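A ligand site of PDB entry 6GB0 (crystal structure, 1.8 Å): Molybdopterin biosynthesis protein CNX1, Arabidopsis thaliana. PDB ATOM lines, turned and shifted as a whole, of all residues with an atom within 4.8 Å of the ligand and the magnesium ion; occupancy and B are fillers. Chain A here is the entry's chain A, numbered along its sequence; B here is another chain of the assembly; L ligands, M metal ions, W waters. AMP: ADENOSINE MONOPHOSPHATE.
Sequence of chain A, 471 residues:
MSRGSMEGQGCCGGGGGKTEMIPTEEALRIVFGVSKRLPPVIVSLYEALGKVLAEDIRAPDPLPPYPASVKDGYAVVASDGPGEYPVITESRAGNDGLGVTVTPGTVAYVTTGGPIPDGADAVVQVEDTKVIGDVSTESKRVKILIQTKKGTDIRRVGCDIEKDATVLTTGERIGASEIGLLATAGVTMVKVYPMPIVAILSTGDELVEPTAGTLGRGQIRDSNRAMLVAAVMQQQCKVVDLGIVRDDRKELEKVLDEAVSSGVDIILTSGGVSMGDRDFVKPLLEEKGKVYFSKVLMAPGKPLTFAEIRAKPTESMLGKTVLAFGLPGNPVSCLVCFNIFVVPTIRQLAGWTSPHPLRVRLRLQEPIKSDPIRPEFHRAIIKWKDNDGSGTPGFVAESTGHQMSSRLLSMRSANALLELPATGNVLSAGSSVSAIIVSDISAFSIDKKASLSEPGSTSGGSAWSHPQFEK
Merely in contact with the magnesium ion: Glu 206. Of the 25 residues printed, 1 comes within 4 Å of the magnesium ion.
O of Gly 329 lies close to O4' of the ligand (3.2 Å). Residues that only touch the ligand: Thr 203 (3.8 Å), Leu 207 (3.6 Å), Ile 220 (3.5 Å), Arg 221 (3.99 Å), Gly 271 (3.4 Å), Val 273 (3.9 Å), Thr 112 of chain B (3.5 Å), Gly 113 of chain B (3.4 Å) and Arg 155 of chain B (3.8 Å). Hydrophobic or aromatic side chains that line the ligand: Leu 207 and Ile 220. 18 residues have an atom within 4 Å of the ligand: Ser 202, Thr 203, Glu 206, Leu 207, Ile 220, Arg 221, Asp 222, Ser 223, Asn 224, Gly 271, Gly 272, Val 273, Ser 274, Gly 329, Asn 330, Thr 112 of chain B, Gly 113 of chain B and Arg 155 of chain B.
Water W6 lies within hydrogen-bond range of the side-chain carboxylate (OD1) of Asp 247, the side-chain hydroxyl (OG1) of Thr 203 and the backbone NH (N) of Gly 272. Water W11 bridges OD2 of Asp 247 and OE1 of Glu 206. Water W1 lies within hydrogen-bond range of the backbone carbonyl oxygen of Thr 112 of chain B (3.0 Å), an oxygen (O1P) of the ligand (3.1 Å) and the side-chain carboxylate of Glu 206 (3.2 Å). Water W12 bridges O3' of the ligand and NH1 of Arg 155 of chain B. Water W13 lies within hydrogen-bond range of OD1 of Asn 330 (2.7 Å) and O3' of the ligand (2.8 Å). Water W3 lies within hydrogen-bond range of the side-chain hydroxyl (OG) of Ser 270 (2.7 Å), a nitrogen (N7) of the ligand (2.8 Å) and the backbone NH (N) of Thr 203 (2.8 Å).
The side-chain carboxylate (OE2) of Glu 206 sits at hydrogen-bond distance from an oxygen (O2') of the ligand. N of Gly 272 is in hydrogen-bond range of O3P of the ligand (3.4 Å). The side-chain carboxylate (OD1) of Asp 222 lies within hydrogen-bond range of a nitrogen (N6) of the ligand (2.8 Å). O3P of the ligand lies within hydrogen-bond range of OG of Ser 274 (2.9 Å). The backbone NH (N) of Asn 330 sits at hydrogen-bond distance from an oxygen (O4') of the ligand, 3.1 Å away. The backbone NH (N) of Ser 223 sits at hydrogen-bond distance from a nitrogen (N1) of the ligand (3.2 Å). A nitrogen (N1) of the ligand sits close to the side-chain hydroxyl of Ser 223, 3.4 Å away. N of Asn 224 lies within hydrogen-bond range of N1 of the ligand (3.4 Å). The side-chain hydroxyl of Ser 202 is in hydrogen-bond range of a nitrogen (N6) of the ligand (3.5 Å).
The magnesium ion is bound by water W11. An oxygen (O2P) of the ligand is bound to the magnesium ion, 2.1 Å away. The magnesium ion is bound by water W6 (2.1 Å). Water W1 binds the magnesium ion (2.1 Å). The magnesium ion is bound by water W7 (2.1 Å). Water W2 binds the magnesium ion, 2.1 Å away.
O of Glu 206 lies within hydrogen-bond range of N of Ile 220, at 3.0 Å. The backbone NH (N) of Gly 272 lies within hydrogen-bond range of the side-chain hydroxyl (OG1) of Thr 203 (3.4 Å). The side-chain hydroxyl (OG) of Ser 202 sits at hydrogen-bond distance from the side-chain carboxylate (OD1) of Asp 222. The guanidinium group of Arg 225 is in salt-bridge range of the side-chain carboxylate of Asp 222, 2.7 Å away. The side-chain hydroxyl (OG) of Ser 270 sits at hydrogen-bond distance from the side-chain amide nitrogen (ND2) of Asn 224 (3.1 Å). OG1 of Thr 203 sits close to O of Gly 271, at 3.5 Å. The backbone NH (N) of Thr 112 of chain B sits at hydrogen-bond distance from the side-chain carboxylate (OD1) of Asp 72 of chain B. The side-chain hydroxyl (OG1) of Thr 203 lies within hydrogen-bond range of the backbone carbonyl oxygen (O) of Ser 270 (2.9 Å).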
ATOM      1  N   SER A 202      -4.234 -15.456   4.136  1.00  0.00           N
ATOM      2  CA  SER A 202      -3.541 -15.566   2.854  1.00  0.00           C
ATOM      3  C   SER A 202      -4.420 -16.365   1.911  1.00  0.00           C
ATOM      4  O   SER A 202      -5.207 -17.200   2.365  1.00  0.00           O
ATOM      5  CB  SER A 202      -2.203 -16.270   3.020  1.00  0.00           C
ATOM      6  OG  SER A 202      -1.294 -15.362   3.618  1.00  0.00           O
ATOM      7  N   THR A 203      -4.291 -16.123   0.605  1.00  0.00           N
ATOM      8  CA  THR A 203      -5.052 -16.893  -0.376  1.00  0.00           C
ATOM      9  C   THR A 203      -4.122 -17.526  -1.408  1.00  0.00           C
ATOM     10  O   THR A 203      -3.156 -16.896  -1.861  1.00  0.00           O
ATOM     11  CB  THR A 203      -6.146 -16.052  -1.121  1.00  0.00           C
ATOM     12  OG1 THR A 203      -5.526 -15.160  -2.042  1.00  0.00           O
ATOM     13  CG2 THR A 203      -7.081 -15.312  -0.170  1.00  0.00           C
ATOM     14  N   GLY A 204      -4.485 -18.719  -1.858  1.00  0.00           N
ATOM     15  CA  GLY A 204      -3.759 -19.359  -2.932  1.00  0.00           C
ATOM     16  C   GLY A 204      -3.679 -20.860  -2.842  1.00  0.00           C
ATOM     17  O   GLY A 204      -3.235 -21.408  -1.828  1.00  0.00           O
ATOM     18  N   GLU A 206      -1.457 -22.425  -4.535  1.00  0.00           N
ATOM     19  CA  GLU A 206      -0.005 -22.654  -4.597  1.00  0.00           C
ATOM     20  C   GLU A 206       0.683 -22.536  -3.205  1.00  0.00           C
ATOM     21  O   GLU A 206       1.836 -22.937  -3.079  1.00  0.00           O
ATOM     22  CB  GLU A 206       0.680 -21.716  -5.634  1.00  0.00           C
ATOM     23  CG  GLU A 206       0.989 -20.273  -5.212  1.00  0.00           C
ATOM     24  CD  GLU A 206      -0.182 -19.313  -5.077  1.00  0.00           C
ATOM     25  OE1 GLU A 206      -1.350 -19.763  -5.095  1.00  0.00           O
ATOM     26  OE2 GLU A 206       0.068 -18.098  -4.943  1.00  0.00           O
ATOM     27  N   LEU A 207       0.007 -22.015  -2.188  1.00  0.00           N
ATOM     28  CA  LEU A 207       0.602 -21.838  -0.863  1.00  0.00           C
ATOM     29  C   LEU A 207       0.676 -23.079  -0.001  1.00  0.00           C
ATOM     30  O   LEU A 207      -0.283 -23.864   0.052  1.00  0.00           O
ATOM     31  CB  LEU A 207      -0.170 -20.761  -0.067  1.00  0.00           C
ATOM     32  CG  LEU A 207      -0.325 -19.374  -0.721  1.00  0.00           C
ATOM     33  CD1 LEU A 207      -1.055 -18.421   0.259  1.00  0.00           C
ATOM     34  CD2 LEU A 207       1.049 -18.788  -1.159  1.00  0.00           C
ATOM     35  N   ILE A 220       4.865 -22.661  -3.017  1.00  0.00           N
ATOM     36  CA  ILE A 220       5.732 -21.691  -2.361  1.00  0.00           C
ATOM     37  C   ILE A 220       5.231 -21.603  -0.935  1.00  0.00           C
ATOM     38  O   ILE A 220       4.045 -21.831  -0.679  1.00  0.00           O
ATOM     39  CB  ILE A 220       5.738 -20.278  -3.042  1.00  0.00           C
ATOM     40  CG1 ILE A 220       4.319 -19.603  -2.982  1.00  0.00           C
ATOM     41  CG2 ILE A 220       6.230 -20.386  -4.467  1.00  0.00           C
ATOM     42  CD1 ILE A 220       4.280 -18.156  -3.432  1.00  0.00           C
ATOM     43  N   ARG A 221       6.112 -21.209  -0.017  1.00  0.00           N
ATOM     44  CA  ARG A 221       5.694 -20.994   1.371  1.00  0.00           C
ATOM     45  C   ARG A 221       4.904 -19.694   1.478  1.00  0.00           C
ATOM     46  O   ARG A 221       5.218 -18.694   0.817  1.00  0.00           O
ATOM     47  CB  ARG A 221       6.915 -20.939   2.306  1.00  0.00           C
ATOM     48  CG  ARG A 221       7.617 -22.288   2.367  1.00  0.00           C
ATOM     49  CD  ARG A 221       8.720 -22.395   3.437  1.00  0.00           C
ATOM     50  NE  ARG A 221       9.480 -23.620   3.200  1.00  0.00           N
ATOM     51  CZ  ARG A 221      10.428 -23.761   2.280  1.00  0.00           C
ATOM     52  NH1 ARG A 221      10.818 -22.723   1.541  1.00  0.00           N
ATOM     53  NH2 ARG A 221      11.009 -24.942   2.097  1.00  0.00           N
ATOM     54  N   ASP A 222       3.851 -19.721   2.299  1.00  0.00           N
ATOM     55  CA  ASP A 222       3.076 -18.523   2.602  1.00  0.00           C
ATOM     56  C   ASP A 222       4.021 -17.578   3.423  1.00  0.00           C
ATOM     57  O   ASP A 222       4.331 -17.873   4.581  1.00  0.00           O
ATOM     58  CB  ASP A 222       1.871 -18.921   3.456  1.00  0.00           C
ATOM     59  CG  ASP A 222       0.986 -17.797   3.932  1.00  0.00           C
ATOM     60  OD1 ASP A 222       1.232 -16.641   3.543  1.00  0.00           O
ATOM     61  OD2 ASP A 222       0.049 -18.076   4.693  1.00  0.00           O
ATOM     62  N   SER A 223       4.512 -16.475   2.804  1.00  0.00           N
ATOM     63  CA  SER A 223       5.360 -15.484   3.495  1.00  0.00           C
ATOM     64  C   SER A 223       4.538 -14.236   3.912  1.00  0.00           C
ATOM     65  O   SER A 223       4.848 -13.609   4.918  1.00  0.00           O
ATOM     66  CB  SER A 223       6.550 -15.081   2.615  1.00  0.00           C
ATOM     67  OG  SER A 223       6.126 -14.476   1.409  1.00  0.00           O
ATOM     68  N   ASN A 224       3.518 -13.884   3.155  1.00  0.00           N
ATOM     69  CA  ASN A 224       2.710 -12.699   3.432  1.00  0.00           C
ATOM     70  C   ASN A 224       2.015 -12.696   4.770  1.00  0.00           C
ATOM     71  O   ASN A 224       1.951 -11.637   5.416  1.00  0.00           O
ATOM     72  CB  ASN A 224       1.649 -12.469   2.304  1.00  0.00           C
ATOM     73  CG  ASN A 224       2.206 -11.933   1.021  1.00  0.00           C
ATOM     74  OD1 ASN A 224       3.376 -11.556   0.932  1.00  0.00           O
ATOM     75  ND2 ASN A 224       1.391 -11.862  -0.021  1.00  0.00           N
ATOM     76  N   ARG A 225       1.462 -13.862   5.185  1.00  0.00           N
ATOM     77  CA  ARG A 225       0.711 -13.912   6.418  1.00  0.00           C
ATOM     78  C   ARG A 225       1.604 -13.592   7.608  1.00  0.00           C
ATOM     79  O   ARG A 225       1.271 -12.672   8.359  1.00  0.00           O
ATOM     80  CB  ARG A 225       0.009 -15.259   6.600  1.00  0.00           C
ATOM     81  CG  ARG A 225      -0.960 -15.330   7.777  1.00  0.00           C
ATOM     82  CD  ARG A 225      -1.970 -16.443   7.519  1.00  0.00           C
ATOM     83  NE  ARG A 225      -1.277 -17.648   7.059  1.00  0.00           N
ATOM     84  CZ  ARG A 225      -0.869 -18.678   7.802  1.00  0.00           C
ATOM     85  NH1 ARG A 225      -1.163 -18.736   9.106  1.00  0.00           N
ATOM     86  NH2 ARG A 225      -0.189 -19.670   7.253  1.00  0.00           N
ATOM     87  N   ASP A 247      -8.324 -21.051  -3.405  1.00  0.00           N
ATOM     88  CA  ASP A 247      -8.978 -20.257  -4.445  1.00  0.00           C
ATOM     89  C   ASP A 247     -10.336 -20.866  -4.778  1.00  0.00           C
ATOM     90  O   ASP A 247     -10.570 -21.364  -5.884  1.00  0.00           O
ATOM     91  CB  ASP A 247      -8.047 -20.089  -5.670  1.00  0.00           C
ATOM     92  CG  ASP A 247      -6.719 -19.429  -5.307  1.00  0.00           C
ATOM     93  OD1 ASP A 247      -6.725 -18.466  -4.498  1.00  0.00           O
ATOM     94  OD2 ASP A 247      -5.685 -19.891  -5.802  1.00  0.00           O
ATOM     95  N   SER A 270      -4.493 -11.149   1.317  1.00  0.00           N
ATOM     96  CA  SER A 270      -3.454 -10.878   0.316  1.00  0.00           C
ATOM     97  C   SER A 270      -3.666 -11.893  -0.828  1.00  0.00           C
ATOM     98  O   SER A 270      -4.202 -12.969  -0.580  1.00  0.00           O
ATOM     99  CB  SER A 270      -2.040 -10.903   0.899  1.00  0.00           C
ATOM    100  OG  SER A 270      -1.482 -12.199   1.017  1.00  0.00           O
ATOM    101  N   GLY A 271      -3.393 -11.482  -2.060  1.00  0.00           N
ATOM    102  CA  GLY A 271      -3.623 -12.320  -3.233  1.00  0.00           C
ATOM    103  C   GLY A 271      -5.098 -12.393  -3.618  1.00  0.00           C
ATOM    104  O   GLY A 271      -5.951 -11.823  -2.931  1.00  0.00           O
ATOM    105  N   GLY A 272      -5.400 -13.100  -4.716  1.00  0.00           N
ATOM    106  CA  GLY A 272      -6.760 -13.267  -5.202  1.00  0.00           C
ATOM    107  C   GLY A 272      -7.451 -11.980  -5.604  1.00  0.00           C
ATOM    108  O   GLY A 272      -8.678 -11.892  -5.524  1.00  0.00           O
ATOM    109  N   VAL A 273      -6.660 -10.951  -6.004  1.00  0.00           N
ATOM    110  CA  VAL A 273      -7.147  -9.609  -6.371  1.00  0.00           C
ATOM    111  C   VAL A 273      -6.581  -9.166  -7.726  1.00  0.00           C
ATOM    112  O   VAL A 273      -6.683  -7.995  -8.007  1.00  0.00           O
ATOM    113  CB  VAL A 273      -6.848  -8.514  -5.272  1.00  0.00           C
ATOM    114  CG1 VAL A 273      -7.847  -8.571  -4.138  1.00  0.00           C
ATOM    115  CG2 VAL A 273      -5.423  -8.616  -4.736  1.00  0.00           C
ATOM    116  N   SER A 274      -5.985 -10.052  -8.563  1.00  0.00           N
ATOM    117  CA  SER A 274      -5.480  -9.628  -9.878  1.00  0.00           C
ATOM    118  C   SER A 274      -6.565  -9.992 -10.921  1.00  0.00           C
ATOM    119  O   SER A 274      -7.766  -9.921 -10.629  1.00  0.00           O
ATOM    120  CB  SER A 274      -4.130 -10.275 -10.189  1.00  0.00           C
ATOM    121  OG  SER A 274      -3.197 -10.190  -9.136  1.00  0.00           O
ATOM    122  N   ASP A 279      -9.701 -15.420  -8.753  1.00  0.00           N
ATOM    123  CA  ASP A 279      -9.382 -14.297  -7.852  1.00  0.00           C
ATOM    124  C   ASP A 279     -10.740 -13.788  -7.356  1.00  0.00           C
ATOM    125  O   ASP A 279     -11.397 -13.017  -8.059  1.00  0.00           O
ATOM    126  CB  ASP A 279      -8.605 -13.202  -8.639  1.00  0.00           C
ATOM    127  CG  ASP A 279      -7.123 -13.517  -8.862  1.00  0.00           C
ATOM    128  OD1 ASP A 279      -6.644 -14.533  -8.335  1.00  0.00           O
ATOM    129  OD2 ASP A 279      -6.448 -12.739  -9.534  1.00  0.00           O
ATOM    130  N   GLY A 329      -0.958  -9.889  -3.769  1.00  0.00           N
ATOM    131  CA  GLY A 329      -0.218 -11.096  -3.387  1.00  0.00           C
ATOM    132  C   GLY A 329       1.280 -10.924  -3.448  1.00  0.00           C
ATOM    133  O   GLY A 329       1.998 -11.526  -2.642  1.00  0.00           O
ATOM    134  N   ASN A 330       1.789 -10.139  -4.423  1.00  0.00           N
ATOM    135  CA  ASN A 330       3.228  -9.915  -4.573  1.00  0.00           C
ATOM    136  C   ASN A 330       3.811  -9.400  -3.251  1.00  0.00           C
ATOM    137  O   ASN A 330       3.295  -8.405  -2.739  1.00  0.00           O
ATOM    138  CB  ASN A 330       3.530  -8.947  -5.725  1.00  0.00           C
ATOM    139  CG  ASN A 330       3.501  -9.647  -7.059  1.00  0.00           C
ATOM    140  OD1 ASN A 330       4.149 -10.701  -7.256  1.00  0.00           O
ATOM    141  ND2 ASN A 330       2.731  -9.131  -7.996  1.00  0.00           N
ATOM    142  N   PRO A 331       4.773 -10.114  -2.626  1.00  0.00           N
ATOM    143  CA  PRO A 331       5.254  -9.724  -1.277  1.00  0.00           C
ATOM    144  C   PRO A 331       5.613  -8.266  -1.069  1.00  0.00           C
ATOM    145  O   PRO A 331       5.292  -7.703  -0.030  1.00  0.00           O
ATOM    146  CB  PRO A 331       6.481 -10.626  -1.084  1.00  0.00           C
ATOM    147  CG  PRO A 331       6.103 -11.861  -1.767  1.00  0.00           C
ATOM    148  CD  PRO A 331       5.419 -11.383  -3.042  1.00  0.00           C
ATOM    149  N   ASP B  72      -1.731 -12.898 -15.366  1.00  0.00           N
ATOM    150  CA  ASP B  72      -2.903 -13.708 -15.665  1.00  0.00           C
ATOM    151  C   ASP B  72      -3.060 -13.559 -17.167  1.00  0.00           C
ATOM    152  O   ASP B  72      -3.170 -12.437 -17.666  1.00  0.00           O
ATOM    153  CB  ASP B  72      -4.144 -13.176 -14.942  1.00  0.00           C
ATOM    154  CG  ASP B  72      -3.911 -13.047 -13.457  1.00  0.00           C
ATOM    155  OD1 ASP B  72      -3.857 -14.091 -12.791  1.00  0.00           O
ATOM    156  OD2 ASP B  72      -3.744 -11.919 -12.989  1.00  0.00           O
ATOM    157  N   THR B 112      -1.287 -15.432 -12.352  1.00  0.00           N
ATOM    158  CA  THR B 112      -0.044 -14.935 -11.749  1.00  0.00           C
ATOM    159  C   THR B 112       0.398 -15.926 -10.665  1.00  0.00           C
ATOM    160  O   THR B 112      -0.436 -16.395  -9.884  1.00  0.00           O
ATOM    161  CB  THR B 112      -0.227 -13.531 -11.163  1.00  0.00           C
ATOM    162  OG1 THR B 112      -0.725 -12.673 -12.195  1.00  0.00           O
ATOM    163  CG2 THR B 112       1.083 -12.956 -10.567  1.00  0.00           C
ATOM    164  N   GLY B 113       1.666 -16.318 -10.707  1.00  0.00           N
ATOM    165  CA  GLY B 113       2.224 -17.295  -9.781  1.00  0.00           C
ATOM    166  C   GLY B 113       2.038 -18.727 -10.243  1.00  0.00           C
ATOM    167  O   GLY B 113       2.574 -19.637  -9.609  1.00  0.00           O
ATOM    168  N   ARG B 155       8.975 -15.393 -14.327  1.00  0.00           N
ATOM    169  CA  ARG B 155       9.988 -15.329 -13.277  1.00  0.00           C
ATOM    170  C   ARG B 155      10.691 -16.685 -13.343  1.00  0.00           C
ATOM    171  O   ARG B 155      10.096 -17.680 -12.965  1.00  0.00           O
ATOM    172  CB  ARG B 155       9.332 -15.163 -11.903  1.00  0.00           C
ATOM    173  CG  ARG B 155       8.796 -13.772 -11.667  1.00  0.00           C
ATOM    174  CD  ARG B 155       7.727 -13.808 -10.578  1.00  0.00           C
ATOM    175  NE  ARG B 155       8.308 -14.246  -9.310  1.00  0.00           N
ATOM    176  CZ  ARG B 155       7.744 -15.068  -8.414  1.00  0.00           C
ATOM    177  NH1 ARG B 155       6.542 -15.570  -8.636  1.00  0.00           N
ATOM    178  NH2 ARG B 155       8.388 -15.381  -7.302  1.00  0.00           N
HETATM  179  P   AMP L   1      -2.474 -13.347  -6.870  1.00  0.00           P
HETATM  180  O1P AMP L   1      -2.302 -13.855  -8.304  1.00  0.00           O
HETATM  181  O2P AMP L   1      -3.212 -14.293  -5.967  1.00  0.00           O
HETATM  182  O3P AMP L   1      -2.966 -11.931  -6.796  1.00  0.00           O
HETATM  183  O5' AMP L   1      -0.958 -13.302  -6.315  1.00  0.00           O
HETATM  184  C5' AMP L   1       0.044 -12.541  -6.997  1.00  0.00           C
HETATM  185  C4' AMP L   1       1.422 -13.138  -6.759  1.00  0.00           C
HETATM  186  O4' AMP L   1       1.725 -13.120  -5.362  1.00  0.00           O
HETATM  187  C3' AMP L   1       1.609 -14.595  -7.204  1.00  0.00           C
HETATM  188  O3' AMP L   1       2.938 -14.695  -7.747  1.00  0.00           O
HETATM  189  C2' AMP L   1       1.463 -15.390  -5.923  1.00  0.00           C
HETATM  190  O2' AMP L   1       2.114 -16.666  -5.895  1.00  0.00           O
HETATM  191  C1' AMP L   1       2.061 -14.432  -4.898  1.00  0.00           C
HETATM  192  N9  AMP L   1       1.500 -14.658  -3.552  1.00  0.00           N
HETATM  193  C8  AMP L   1       0.193 -14.671  -3.236  1.00  0.00           C
HETATM  194  N7  AMP L   1       0.038 -14.915  -1.916  1.00  0.00           N
HETATM  195  C5  AMP L   1       1.262 -15.022  -1.376  1.00  0.00           C
HETATM  196  C6  AMP L   1       1.811 -15.318  -0.042  1.00  0.00           C
HETATM  197  N6  AMP L   1       0.985 -15.490   0.988  1.00  0.00           N
HETATM  198  N1  AMP L   1       3.152 -15.351   0.133  1.00  0.00           N
HETATM  199  C2  AMP L   1       3.985 -15.200  -0.920  1.00  0.00           C
HETATM  200  N3  AMP L   1       3.557 -14.945  -2.176  1.00  0.00           N
HETATM  201  C4  AMP L   1       2.228 -14.858  -2.458  1.00  0.00           C
HETATM  202 MG    MG M   1      -3.381 -16.343  -5.950  1.00  0.00          MG
HETATM  203  O   HOH W   1      -1.725 -16.653  -7.163  1.00  0.00           O
HETATM  204  O   HOH W   2      -4.769 -16.262  -7.509  1.00  0.00           O
HETATM  205  O   HOH W   3      -1.873 -14.725   0.128  1.00  0.00           O
HETATM  206  O   HOH W   4       7.458 -15.410  -0.895  1.00  0.00           O
HETATM  207  O   HOH W   5      -2.216  -9.474  -6.183  1.00  0.00           O
HETATM  208  O   HOH W   6      -4.901 -16.331  -4.554  1.00  0.00           O
HETATM  209  O   HOH W   7      -1.998 -16.520  -4.399  1.00  0.00           O
HETATM  210  O   HOH W   8       4.653 -17.512  -7.129  1.00  0.00           O
HETATM  211  O   HOH W   9      -4.119 -14.035 -10.133  1.00  0.00           O
HETATM  212  O   HOH W  10       6.122 -15.025  -3.260  1.00  0.00           O
HETATM  213  O   HOH W  11      -3.483 -18.384  -6.180  1.00  0.00           O
HETATM  214  O   HOH W  12       4.421 -14.263 -10.032  1.00  0.00           O
HETATM  215  O   HOH W  13       4.954 -13.209  -6.577  1.00  0.00           O
